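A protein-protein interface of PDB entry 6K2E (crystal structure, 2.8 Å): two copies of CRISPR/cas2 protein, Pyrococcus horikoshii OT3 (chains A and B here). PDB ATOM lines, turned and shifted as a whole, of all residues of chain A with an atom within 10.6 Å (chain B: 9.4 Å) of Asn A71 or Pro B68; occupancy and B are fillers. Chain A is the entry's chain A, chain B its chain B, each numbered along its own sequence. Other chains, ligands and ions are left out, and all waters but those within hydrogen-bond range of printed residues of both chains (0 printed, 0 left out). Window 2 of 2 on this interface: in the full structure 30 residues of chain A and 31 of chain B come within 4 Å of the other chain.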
ATOM      1  N   HIS A   3     -34.940  16.048  25.111  1.00  0.00           N
ATOM      2  CA  HIS A   3     -34.218  16.398  23.904  1.00  0.00           C
ATOM      3  C   HIS A   3     -33.156  17.459  24.155  1.00  0.00           C
ATOM      4  O   HIS A   3     -33.285  18.314  25.045  1.00  0.00           O
ATOM      5  CB  HIS A   3     -35.195  16.835  22.822  1.00  0.00           C
ATOM      6  CG  HIS A   3     -35.551  15.723  21.899  1.00  0.00           C
ATOM      7  ND1 HIS A   3     -36.107  14.549  22.347  1.00  0.00           N
ATOM      8  CD2 HIS A   3     -35.332  15.557  20.574  1.00  0.00           C
ATOM      9  CE1 HIS A   3     -36.261  13.723  21.329  1.00  0.00           C
ATOM     10  NE2 HIS A   3     -35.794  14.309  20.242  1.00  0.00           N
ATOM     11  N   MET A   4     -32.075  17.352  23.383  1.00  0.00           N
ATOM     12  CA  MET A   4     -30.958  18.281  23.442  1.00  0.00           C
ATOM     13  C   MET A   4     -30.635  18.769  22.039  1.00  0.00           C
ATOM     14  O   MET A   4     -31.072  18.188  21.046  1.00  0.00           O
ATOM     15  CB  MET A   4     -29.692  17.655  24.052  1.00  0.00           C
ATOM     16  CG  MET A   4     -29.677  17.550  25.576  1.00  0.00           C
ATOM     17  SD  MET A   4     -30.278  15.978  26.152  1.00  0.00           S
ATOM     18  CE  MET A   4     -29.330  14.911  25.064  1.00  0.00           C
ATOM     19  N   TYR A   5     -29.913  19.882  21.967  1.00  0.00           N
ATOM     20  CA  TYR A   5     -29.314  20.341  20.719  1.00  0.00           C
ATOM     21  C   TYR A   5     -27.799  20.156  20.780  1.00  0.00           C
ATOM     22  O   TYR A   5     -27.184  20.423  21.814  1.00  0.00           O
ATOM     23  CB  TYR A   5     -29.668  21.810  20.449  1.00  0.00           C
ATOM     24  CG  TYR A   5     -29.505  22.209  19.007  1.00  0.00           C
ATOM     25  CD1 TYR A   5     -28.310  22.770  18.534  1.00  0.00           C
ATOM     26  CD2 TYR A   5     -30.530  22.017  18.109  1.00  0.00           C
ATOM     27  CE1 TYR A   5     -28.164  23.120  17.195  1.00  0.00           C
ATOM     28  CE2 TYR A   5     -30.394  22.378  16.775  1.00  0.00           C
ATOM     29  CZ  TYR A   5     -29.218  22.912  16.326  1.00  0.00           C
ATOM     30  OH  TYR A   5     -29.124  23.245  15.005  1.00  0.00           O
ATOM     31  N   VAL A   6     -27.186  19.731  19.668  1.00  0.00           N
ATOM     32  CA  VAL A   6     -25.740  19.511  19.661  1.00  0.00           C
ATOM     33  C   VAL A   6     -25.080  20.253  18.507  1.00  0.00           C
ATOM     34  O   VAL A   6     -25.684  20.462  17.454  1.00  0.00           O
ATOM     35  CB  VAL A   6     -25.350  18.015  19.608  1.00  0.00           C
ATOM     36  CG1 VAL A   6     -25.630  17.344  20.936  1.00  0.00           C
ATOM     37  CG2 VAL A   6     -26.062  17.315  18.492  1.00  0.00           C
ATOM     38  N   ILE A   7     -23.825  20.657  18.722  1.00  0.00           N
ATOM     39  CA  ILE A   7     -22.938  21.167  17.674  1.00  0.00           C
ATOM     40  C   ILE A   7     -21.683  20.315  17.719  1.00  0.00           C
ATOM     41  O   ILE A   7     -21.064  20.182  18.779  1.00  0.00           O
ATOM     42  CB  ILE A   7     -22.562  22.650  17.856  1.00  0.00           C
ATOM     43  CG1 ILE A   7     -23.771  23.559  17.832  1.00  0.00           C
ATOM     44  CG2 ILE A   7     -21.623  23.113  16.746  1.00  0.00           C
ATOM     45  CD1 ILE A   7     -23.393  24.993  18.192  1.00  0.00           C
ATOM     46  N   GLU A  37     -24.814  19.960  13.098  1.00  0.00           N
ATOM     47  CA  GLU A  37     -25.651  20.376  14.215  1.00  0.00           C
ATOM     48  C   GLU A  37     -27.061  19.830  14.054  1.00  0.00           C
ATOM     49  O   GLU A  37     -27.444  19.354  12.985  1.00  0.00           O
ATOM     50  CB  GLU A  37     -25.673  21.905  14.371  1.00  0.00           C
ATOM     51  CG  GLU A  37     -26.001  22.662  13.106  1.00  0.00           C
ATOM     52  CD  GLU A  37     -25.936  24.164  13.284  1.00  0.00           C
ATOM     53  OE1 GLU A  37     -26.612  24.696  14.187  1.00  0.00           O
ATOM     54  OE2 GLU A  37     -25.223  24.818  12.504  1.00  0.00           O
ATOM     55  N   GLY A  38     -27.814  19.871  15.141  1.00  0.00           N
ATOM     56  CA  GLY A  38     -29.212  19.490  15.106  1.00  0.00           C
ATOM     57  C   GLY A  38     -29.691  18.927  16.429  1.00  0.00           C
ATOM     58  O   GLY A  38     -28.925  18.713  17.367  1.00  0.00           O
ATOM     59  N   GLU A  39     -30.990  18.644  16.461  1.00  0.00           N
ATOM     60  CA  GLU A  39     -31.624  18.051  17.626  1.00  0.00           C
ATOM     61  C   GLU A  39     -31.352  16.556  17.691  1.00  0.00           C
ATOM     62  O   GLU A  39     -31.370  15.854  16.678  1.00  0.00           O
ATOM     63  CB  GLU A  39     -33.128  18.258  17.560  1.00  0.00           C
ATOM     64  CG  GLU A  39     -33.681  19.494  18.205  1.00  0.00           C
ATOM     65  CD  GLU A  39     -35.176  19.372  18.339  1.00  0.00           C
ATOM     66  OE1 GLU A  39     -35.910  20.148  17.690  1.00  0.00           O
ATOM     67  OE2 GLU A  39     -35.607  18.450  19.068  1.00  0.00           O
ATOM     68  N   ILE A  66     -23.136  20.013  23.900  1.00  0.00           N
ATOM     69  CA  ILE A  66     -24.513  19.599  24.187  1.00  0.00           C
ATOM     70  C   ILE A  66     -25.263  20.737  24.885  1.00  0.00           C
ATOM     71  O   ILE A  66     -24.871  21.164  25.979  1.00  0.00           O
ATOM     72  CB  ILE A  66     -24.539  18.324  25.044  1.00  0.00           C
ATOM     73  CG1 ILE A  66     -23.683  17.231  24.387  1.00  0.00           C
ATOM     74  CG2 ILE A  66     -25.961  17.859  25.223  1.00  0.00           C
ATOM     75  CD1 ILE A  66     -22.624  16.643  25.272  1.00  0.00           C
ATOM     76  N   PHE A  67     -26.374  21.194  24.282  1.00  0.00           N
ATOM     77  CA  PHE A  67     -27.185  22.331  24.736  1.00  0.00           C
ATOM     78  C   PHE A  67     -28.590  21.883  25.139  1.00  0.00           C
ATOM     79  O   PHE A  67     -29.117  20.906  24.588  1.00  0.00           O
ATOM     80  CB  PHE A  67     -27.320  23.411  23.647  1.00  0.00           C
ATOM     81  CG  PHE A  67     -26.020  23.869  23.106  1.00  0.00           C
ATOM     82  CD1 PHE A  67     -25.453  23.252  21.984  1.00  0.00           C
ATOM     83  CD2 PHE A  67     -25.343  24.905  23.715  1.00  0.00           C
ATOM     84  CE1 PHE A  67     -24.234  23.660  21.493  1.00  0.00           C
ATOM     85  CE2 PHE A  67     -24.109  25.303  23.236  1.00  0.00           C
ATOM     86  CZ  PHE A  67     -23.566  24.693  22.108  1.00  0.00           C
ATOM     87  N   PRO A  68     -29.235  22.588  26.081  1.00  0.00           N
ATOM     88  CA  PRO A  68     -30.647  22.281  26.382  1.00  0.00           C
ATOM     89  C   PRO A  68     -31.601  22.652  25.258  1.00  0.00           C
ATOM     90  O   PRO A  68     -32.708  22.110  25.216  1.00  0.00           O
ATOM     91  CB  PRO A  68     -30.926  23.098  27.650  1.00  0.00           C
ATOM     92  CG  PRO A  68     -29.928  24.198  27.599  1.00  0.00           C
ATOM     93  CD  PRO A  68     -28.693  23.586  27.015  1.00  0.00           C
ATOM     94  N   GLY A  69     -31.225  23.566  24.370  1.00  0.00           N
ATOM     95  CA  GLY A  69     -32.061  23.900  23.231  1.00  0.00           C
ATOM     96  C   GLY A  69     -31.317  24.762  22.228  1.00  0.00           C
ATOM     97  O   GLY A  69     -30.151  25.123  22.417  1.00  0.00           O
ATOM     98  N   LYS A  70     -32.047  25.147  21.181  1.00  0.00           N
ATOM     99  CA  LYS A  70     -31.518  25.954  20.083  1.00  0.00           C
ATOM    100  C   LYS A  70     -31.746  27.446  20.347  1.00  0.00           C
ATOM    101  O   LYS A  70     -32.493  28.120  19.649  1.00  0.00           O
ATOM    102  CB  LYS A  70     -32.162  25.521  18.769  1.00  0.00           C
ATOM    103  CG  LYS A  70     -31.413  25.884  17.507  1.00  0.00           C
ATOM    104  CD  LYS A  70     -32.318  25.717  16.285  1.00  0.00           C
ATOM    105  CE  LYS A  70     -31.645  26.227  15.007  1.00  0.00           C
ATOM    106  NZ  LYS A  70     -32.208  25.581  13.776  1.00  0.00           N
ATOM    107  N   ASN A  71     -31.132  27.946  21.422  1.00  0.00           N
ATOM    108  CA  ASN A  71     -31.123  29.382  21.730  1.00  0.00           C
ATOM    109  C   ASN A  71     -29.763  29.974  21.358  1.00  0.00           C
ATOM    110  O   ASN A  71     -28.919  30.241  22.213  1.00  0.00           O
ATOM    111  CB  ASN A  71     -31.465  29.644  23.200  1.00  0.00           C
ATOM    112  CG  ASN A  71     -31.642  31.156  23.523  1.00  0.00           C
ATOM    113  OD1 ASN A  71     -31.557  31.557  24.688  1.00  0.00           O
ATOM    114  ND2 ASN A  71     -31.891  31.983  22.497  1.00  0.00           N
ATOM    115  N   PHE A  72     -29.545  30.174  20.062  1.00  0.00           N
ATOM    116  CA  PHE A  72     -28.341  30.865  19.629  1.00  0.00           C
ATOM    117  C   PHE A  72     -28.582  31.522  18.280  1.00  0.00           C
ATOM    118  O   PHE A  72     -29.471  31.128  17.521  1.00  0.00           O
ATOM    119  CB  PHE A  72     -27.119  29.926  19.537  1.00  0.00           C
ATOM    120  CG  PHE A  72     -27.281  28.788  18.564  1.00  0.00           C
ATOM    121  CD1 PHE A  72     -26.923  28.920  17.212  1.00  0.00           C
ATOM    122  CD2 PHE A  72     -27.762  27.570  19.005  1.00  0.00           C
ATOM    123  CE1 PHE A  72     -27.096  27.895  16.326  1.00  0.00           C
ATOM    124  CE2 PHE A  72     -27.920  26.523  18.120  1.00  0.00           C
ATOM    125  CZ  PHE A  72     -27.583  26.691  16.772  1.00  0.00           C
ATOM    126  N   ASP A  73     -27.713  32.474  17.963  1.00  0.00           N
ATOM    127  CA  ASP A  73     -27.538  32.973  16.610  1.00  0.00           C
ATOM    128  C   ASP A  73     -26.194  32.472  16.087  1.00  0.00           C
ATOM    129  O   ASP A  73     -25.265  32.232  16.861  1.00  0.00           O
ATOM    130  CB  ASP A  73     -27.550  34.508  16.552  1.00  0.00           C
ATOM    131  CG  ASP A  73     -28.852  35.117  17.035  1.00  0.00           C
ATOM    132  OD1 ASP A  73     -28.788  36.033  17.886  1.00  0.00           O
ATOM    133  OD2 ASP A  73     -29.932  34.698  16.566  1.00  0.00           O
ATOM    134  N   LEU A  74     -26.104  32.294  14.770  1.00  0.00           N
ATOM    135  CA  LEU A  74     -24.853  31.968  14.099  1.00  0.00           C
ATOM    136  C   LEU A  74     -24.565  33.057  13.078  1.00  0.00           C
ATOM    137  O   LEU A  74     -25.406  33.359  12.225  1.00  0.00           O
ATOM    138  CB  LEU A  74     -24.892  30.598  13.400  1.00  0.00           C
ATOM    139  CG  LEU A  74     -23.826  30.332  12.312  1.00  0.00           C
ATOM    140  CD1 LEU A  74     -22.405  30.108  12.874  1.00  0.00           C
ATOM    141  CD2 LEU A  74     -24.224  29.167  11.421  1.00  0.00           C
ATOM    142  N   SER B   2     -25.955  42.155  27.296  1.00  0.00           N
ATOM    143  CA  SER B   2     -24.699  42.841  26.995  1.00  0.00           C
ATOM    144  C   SER B   2     -23.522  41.866  26.926  1.00  0.00           C
ATOM    145  O   SER B   2     -22.505  42.150  26.269  1.00  0.00           O
ATOM    146  CB  SER B   2     -24.397  43.924  28.036  1.00  0.00           C
ATOM    147  OG  SER B   2     -22.996  44.128  28.196  1.00  0.00           O
ATOM    148  N   HIS B   3     -23.626  40.732  27.626  1.00  0.00           N
ATOM    149  CA  HIS B   3     -22.542  39.765  27.640  1.00  0.00           C
ATOM    150  C   HIS B   3     -23.007  38.431  27.074  1.00  0.00           C
ATOM    151  O   HIS B   3     -24.101  37.949  27.396  1.00  0.00           O
ATOM    152  CB  HIS B   3     -21.985  39.617  29.035  1.00  0.00           C
ATOM    153  CG  HIS B   3     -20.712  40.367  29.211  1.00  0.00           C
ATOM    154  ND1 HIS B   3     -19.477  39.755  29.187  1.00  0.00           N
ATOM    155  CD2 HIS B   3     -20.472  41.696  29.308  1.00  0.00           C
ATOM    156  CE1 HIS B   3     -18.531  40.670  29.302  1.00  0.00           C
ATOM    157  NE2 HIS B   3     -19.109  41.856  29.382  1.00  0.00           N
ATOM    158  N   MET B   4     -22.147  37.825  26.254  1.00  0.00           N
ATOM    159  CA  MET B   4     -22.478  36.590  25.568  1.00  0.00           C
ATOM    160  C   MET B   4     -21.356  35.575  25.659  1.00  0.00           C
ATOM    161  O   MET B   4     -20.193  35.917  25.874  1.00  0.00           O
ATOM    162  CB  MET B   4     -22.763  36.831  24.087  1.00  0.00           C
ATOM    163  CG  MET B   4     -24.177  37.315  23.754  1.00  0.00           C
ATOM    164  SD  MET B   4     -24.238  39.089  23.684  1.00  0.00           S
ATOM    165  CE  MET B   4     -22.998  39.336  22.426  1.00  0.00           C
ATOM    166  N   TYR B   5     -21.713  34.321  25.410  1.00  0.00           N
ATOM    167  CA  TYR B   5     -20.730  33.272  25.201  1.00  0.00           C
ATOM    168  C   TYR B   5     -20.657  32.932  23.723  1.00  0.00           C
ATOM    169  O   TYR B   5     -21.681  32.856  23.036  1.00  0.00           O
ATOM    170  CB  TYR B   5     -21.054  32.008  25.986  1.00  0.00           C
ATOM    171  CG  TYR B   5     -19.835  31.151  26.176  1.00  0.00           C
ATOM    172  CD1 TYR B   5     -18.964  31.394  27.229  1.00  0.00           C
ATOM    173  CD2 TYR B   5     -19.537  30.117  25.296  1.00  0.00           C
ATOM    174  CE1 TYR B   5     -17.835  30.628  27.409  1.00  0.00           C
ATOM    175  CE2 TYR B   5     -18.405  29.343  25.473  1.00  0.00           C
ATOM    176  CZ  TYR B   5     -17.569  29.606  26.537  1.00  0.00           C
ATOM    177  OH  TYR B   5     -16.457  28.858  26.739  1.00  0.00           O
ATOM    178  N   VAL B   6     -19.455  32.686  23.245  1.00  0.00           N
ATOM    179  CA  VAL B   6     -19.287  32.448  21.828  1.00  0.00           C
ATOM    180  C   VAL B   6     -18.498  31.156  21.620  1.00  0.00           C
ATOM    181  O   VAL B   6     -17.679  30.765  22.456  1.00  0.00           O
ATOM    182  CB  VAL B   6     -18.631  33.695  21.190  1.00  0.00           C
ATOM    183  CG1 VAL B   6     -17.131  33.695  21.291  1.00  0.00           C
ATOM    184  CG2 VAL B   6     -19.077  33.866  19.804  1.00  0.00           C
ATOM    185  N   ILE B   7     -18.795  30.456  20.523  1.00  0.00           N
ATOM    186  CA  ILE B   7     -17.991  29.322  20.064  1.00  0.00           C
ATOM    187  C   ILE B   7     -17.627  29.593  18.615  1.00  0.00           C
ATOM    188  O   ILE B   7     -18.514  29.750  17.769  1.00  0.00           O
ATOM    189  CB  ILE B   7     -18.729  27.979  20.161  1.00  0.00           C
ATOM    190  CG1 ILE B   7     -19.099  27.634  21.593  1.00  0.00           C
ATOM    191  CG2 ILE B   7     -17.877  26.861  19.570  1.00  0.00           C
ATOM    192  CD1 ILE B   7     -19.997  26.426  21.653  1.00  0.00           C
ATOM    193  N   GLY B  38     -15.318  31.344  24.593  1.00  0.00           N
ATOM    194  CA  GLY B  38     -15.167  32.208  25.748  1.00  0.00           C
ATOM    195  C   GLY B  38     -16.232  33.287  25.797  1.00  0.00           C
ATOM    196  O   GLY B  38     -17.074  33.420  24.917  1.00  0.00           O
ATOM    197  N   GLU B  39     -16.168  34.061  26.873  1.00  0.00           N
ATOM    198  CA  GLU B  39     -17.072  35.176  27.073  1.00  0.00           C
ATOM    199  C   GLU B  39     -16.631  36.400  26.285  1.00  0.00           C
ATOM    200  O   GLU B  39     -15.439  36.676  26.151  1.00  0.00           O
ATOM    201  CB  GLU B  39     -17.148  35.511  28.555  1.00  0.00           C
ATOM    202  CG  GLU B  39     -18.548  35.560  29.088  1.00  0.00           C
ATOM    203  CD  GLU B  39     -18.566  35.721  30.582  1.00  0.00           C
ATOM    204  OE1 GLU B  39     -17.672  36.433  31.100  1.00  0.00           O
ATOM    205  OE2 GLU B  39     -19.459  35.133  31.235  1.00  0.00           O
ATOM    206  N   LEU B  40     -17.604  37.132  25.761  1.00  0.00           N
ATOM    207  CA  LEU B  40     -17.352  38.377  25.051  1.00  0.00           C
ATOM    208  C   LEU B  40     -18.482  39.358  25.326  1.00  0.00           C
ATOM    209  O   LEU B  40     -19.643  38.962  25.467  1.00  0.00           O
ATOM    210  CB  LEU B  40     -17.240  38.177  23.533  1.00  0.00           C
ATOM    211  CG  LEU B  40     -15.961  37.602  22.944  1.00  0.00           C
ATOM    212  CD1 LEU B  40     -16.058  37.598  21.427  1.00  0.00           C
ATOM    213  CD2 LEU B  40     -14.744  38.367  23.412  1.00  0.00           C
ATOM    214  N   LEU B  45     -17.202  41.403  20.552  1.00  0.00           N
ATOM    215  CA  LEU B  45     -17.608  40.505  19.477  1.00  0.00           C
ATOM    216  C   LEU B  45     -17.688  41.241  18.147  1.00  0.00           C
ATOM    217  O   LEU B  45     -17.308  40.688  17.107  1.00  0.00           O
ATOM    218  CB  LEU B  45     -18.950  39.827  19.809  1.00  0.00           C
ATOM    219  CG  LEU B  45     -19.543  38.857  18.757  1.00  0.00           C
ATOM    220  CD1 LEU B  45     -18.541  37.846  18.222  1.00  0.00           C
ATOM    221  CD2 LEU B  45     -20.693  38.084  19.277  1.00  0.00           C
ATOM    222  N   TYR B  65     -20.760  31.149  16.617  1.00  0.00           N
ATOM    223  CA  TYR B  65     -22.000  30.782  17.297  1.00  0.00           C
ATOM    224  C   TYR B  65     -22.125  31.622  18.565  1.00  0.00           C
ATOM    225  O   TYR B  65     -21.274  31.531  19.452  1.00  0.00           O
ATOM    226  CB  TYR B  65     -22.034  29.292  17.668  1.00  0.00           C
ATOM    227  CG  TYR B  65     -22.218  28.329  16.527  1.00  0.00           C
ATOM    228  CD1 TYR B  65     -23.487  28.045  16.019  1.00  0.00           C
ATOM    229  CD2 TYR B  65     -21.124  27.693  15.963  1.00  0.00           C
ATOM    230  CE1 TYR B  65     -23.655  27.162  14.960  1.00  0.00           C
ATOM    231  CE2 TYR B  65     -21.280  26.811  14.916  1.00  0.00           C
ATOM    232  CZ  TYR B  65     -22.543  26.546  14.419  1.00  0.00           C
ATOM    233  OH  TYR B  65     -22.665  25.672  13.376  1.00  0.00           O
ATOM    234  N   ILE B  66     -23.175  32.435  18.642  1.00  0.00           N
ATOM    235  CA  ILE B  66     -23.393  33.391  19.722  1.00  0.00           C
ATOM    236  C   ILE B  66     -24.540  32.917  20.618  1.00  0.00           C
ATOM    237  O   ILE B  66     -25.679  32.774  20.159  1.00  0.00           O
ATOM    238  CB  ILE B  66     -23.678  34.786  19.152  1.00  0.00           C
ATOM    239  CG1 ILE B  66     -22.628  35.122  18.079  1.00  0.00           C
ATOM    240  CG2 ILE B  66     -23.743  35.811  20.276  1.00  0.00           C
ATOM    241  CD1 ILE B  66     -23.180  35.863  16.886  1.00  0.00           C
ATOM    242  N   PHE B  67     -24.253  32.736  21.910  1.00  0.00           N
ATOM    243  CA  PHE B  67     -25.139  32.209  22.943  1.00  0.00           C
ATOM    244  C   PHE B  67     -25.403  33.275  23.987  1.00  0.00           C
ATOM    245  O   PHE B  67     -24.544  34.125  24.224  1.00  0.00           O
ATOM    246  CB  PHE B  67     -24.512  30.991  23.630  1.00  0.00           C
ATOM    247  CG  PHE B  67     -24.107  29.938  22.675  1.00  0.00           C
ATOM    248  CD1 PHE B  67     -22.827  29.917  22.140  1.00  0.00           C
ATOM    249  CD2 PHE B  67     -25.013  28.994  22.267  1.00  0.00           C
ATOM    250  CE1 PHE B  67     -22.481  28.980  21.234  1.00  0.00           C
ATOM    251  CE2 PHE B  67     -24.664  28.061  21.351  1.00  0.00           C
ATOM    252  CZ  PHE B  67     -23.404  28.037  20.846  1.00  0.00           C
ATOM    253  N   PRO B  68     -26.564  33.249  24.653  1.00  0.00           N
ATOM    254  CA  PRO B  68     -26.779  34.202  25.755  1.00  0.00           C
ATOM    255  C   PRO B  68     -25.918  33.921  26.965  1.00  0.00           C
ATOM    256  O   PRO B  68     -25.697  34.851  27.747  1.00  0.00           O
ATOM    257  CB  PRO B  68     -28.270  34.055  26.076  1.00  0.00           C
ATOM    258  CG  PRO B  68     -28.854  33.378  24.884  1.00  0.00           C
ATOM    259  CD  PRO B  68     -27.783  32.473  24.374  1.00  0.00           C
ATOM    260  N   GLY B  69     -25.430  32.691  27.139  1.00  0.00           N
ATOM    261  CA  GLY B  69     -24.556  32.349  28.254  1.00  0.00           C
ATOM    262  C   GLY B  69     -23.946  30.973  28.099  1.00  0.00           C
ATOM    263  O   GLY B  69     -24.198  30.269  27.120  1.00  0.00           O
ATOM    264  N   LYS B  70     -23.174  30.571  29.120  1.00  0.00           N
ATOM    265  CA  LYS B  70     -22.456  29.286  29.112  1.00  0.00           C
ATOM    266  C   LYS B  70     -23.312  28.194  29.747  1.00  0.00           C
ATOM    267  O   LYS B  70     -22.958  27.597  30.751  1.00  0.00           O
ATOM    268  CB  LYS B  70     -21.117  29.396  29.848  1.00  0.00           C
ATOM    269  CG  LYS B  70     -19.930  28.546  29.243  1.00  0.00           C
ATOM    270  CD  LYS B  70     -19.824  27.049  29.636  1.00  0.00           C
ATOM    271  CE  LYS B  70     -18.516  26.361  29.126  1.00  0.00           C
ATOM    272  NZ  LYS B  70     -18.203  25.009  29.741  1.00  0.00           N
ATOM    273  N   ASN B  71     -24.464  27.934  29.143  1.00  0.00           N
ATOM    274  CA  ASN B  71     -25.330  26.854  29.612  1.00  0.00           C
ATOM    275  C   ASN B  71     -25.193  25.624  28.711  1.00  0.00           C
ATOM    276  O   ASN B  71     -26.123  25.200  28.034  1.00  0.00           O
ATOM    277  CB  ASN B  71     -26.776  27.345  29.688  1.00  0.00           C
ATOM    278  CG  ASN B  71     -27.672  26.400  30.473  1.00  0.00           C
ATOM    279  OD1 ASN B  71     -27.191  25.452  31.102  1.00  0.00           O
ATOM    280  ND2 ASN B  71     -28.982  26.656  30.439  1.00  0.00           N
ATOM    281  N   PHE B  72     -24.026  24.993  28.768  1.00  0.00           N
ATOM    282  CA  PHE B  72     -23.833  23.773  28.001  1.00  0.00           C
ATOM    283  C   PHE B  72     -22.741  22.958  28.648  1.00  0.00           C
ATOM    284  O   PHE B  72     -21.927  23.484  29.404  1.00  0.00           O
ATOM    285  CB  PHE B  72     -23.472  24.038  26.537  1.00  0.00           C
ATOM    286  CG  PHE B  72     -22.216  24.815  26.337  1.00  0.00           C
ATOM    287  CD1 PHE B  72     -20.992  24.165  26.185  1.00  0.00           C
ATOM    288  CD2 PHE B  72     -22.269  26.192  26.226  1.00  0.00           C
ATOM    289  CE1 PHE B  72     -19.844  24.858  26.006  1.00  0.00           C
ATOM    290  CE2 PHE B  72     -21.116  26.912  26.036  1.00  0.00           C
ATOM    291  CZ  PHE B  72     -19.903  26.242  25.913  1.00  0.00           C
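The backbone carbonyl oxygen of Asp A73 sits at hydrogen-bond distance from the backbone NH of Ile B66 (2.8 Å).
The side-chain carboxylate (OE2) of Glu A37 sits at hydrogen-bond distance from the side-chain hydroxyl (OH) of Tyr B65 (2.8 Å).
The backbone carbonyl oxygen (O) of Tyr A5 sits at hydrogen-bond distance from the backbone NH (N) of Phe A67.
OH of Tyr A5 lies within hydrogen-bond range of OE1 of Glu A37, 3.0 Å away.
The backbone carbonyl oxygen of Tyr B5 is in hydrogen-bond range of the backbone NH of Phe B67 (2.8 Å).
The backbone NH of Tyr B65 is in hydrogen-bond range of the backbone carbonyl oxygen of Ile B7, at 2.9 Å.
Tyr B65 touches Ile A7.
Ile A66 touches Phe B72.
Ile B7 touches Phe A67 (CD1 to CZ, 3.99 Å).
CE2 of Phe B67 touches CE2 of Phe A67 (3.4 Å).
Asn B71 touches Pro A68 (O to CD, 3.2 Å).
CD1 of Tyr B65 touches CE1 of Phe A72, at 3.6 Å.
CB of Phe A72 touches O of Ile B66 (3.3 Å).
CB of Phe A72 touches CD2 of Phe B67, 3.6 Å away.
Asp A73 touches Tyr B65.
Tyr B65 touches Leu A74 (CE1 to CD1, 3.8 Å).
Of the printed residues of chain B, Asn A71 touches Pro B68.
Pro B68 touches one residue of chain A.
Of the printed residues of chain A, Phe B72 touches Ile A66 (3.2 Å) and Phe A67 (3.5 Å).
Of the printed residues of chain A, Tyr B65 touches Ile A7, Glu A37, Phe A72, Asp A73 and Leu A74.
Val B6 touches none of the printed residues of chain A.
Gly A38 touches none of the printed residues of chain B.
The nearest residue of chain B that does not touch Asn A71 is Phe B67 (4.1 Å).
Among the printed residues, 14 pairs touch across the chains.
Among the printed residues, no Asp or Glu carboxylate lies within 4 Å of a Lys or Arg side-chain nitrogen of the other chain.
Ile A66 touches Phe B72, and with the chains exchanged Phe A72 touches Ile B66.
Phe A67 touches Ile B7, but with the chains exchanged Ile A7 does not touch Phe B67 (4.04 Å).
Phe A67 touches its own counterpart, Phe B67.
Phe A67 touches Phe B72, and with the chains exchanged Phe A72 touches Phe B67.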
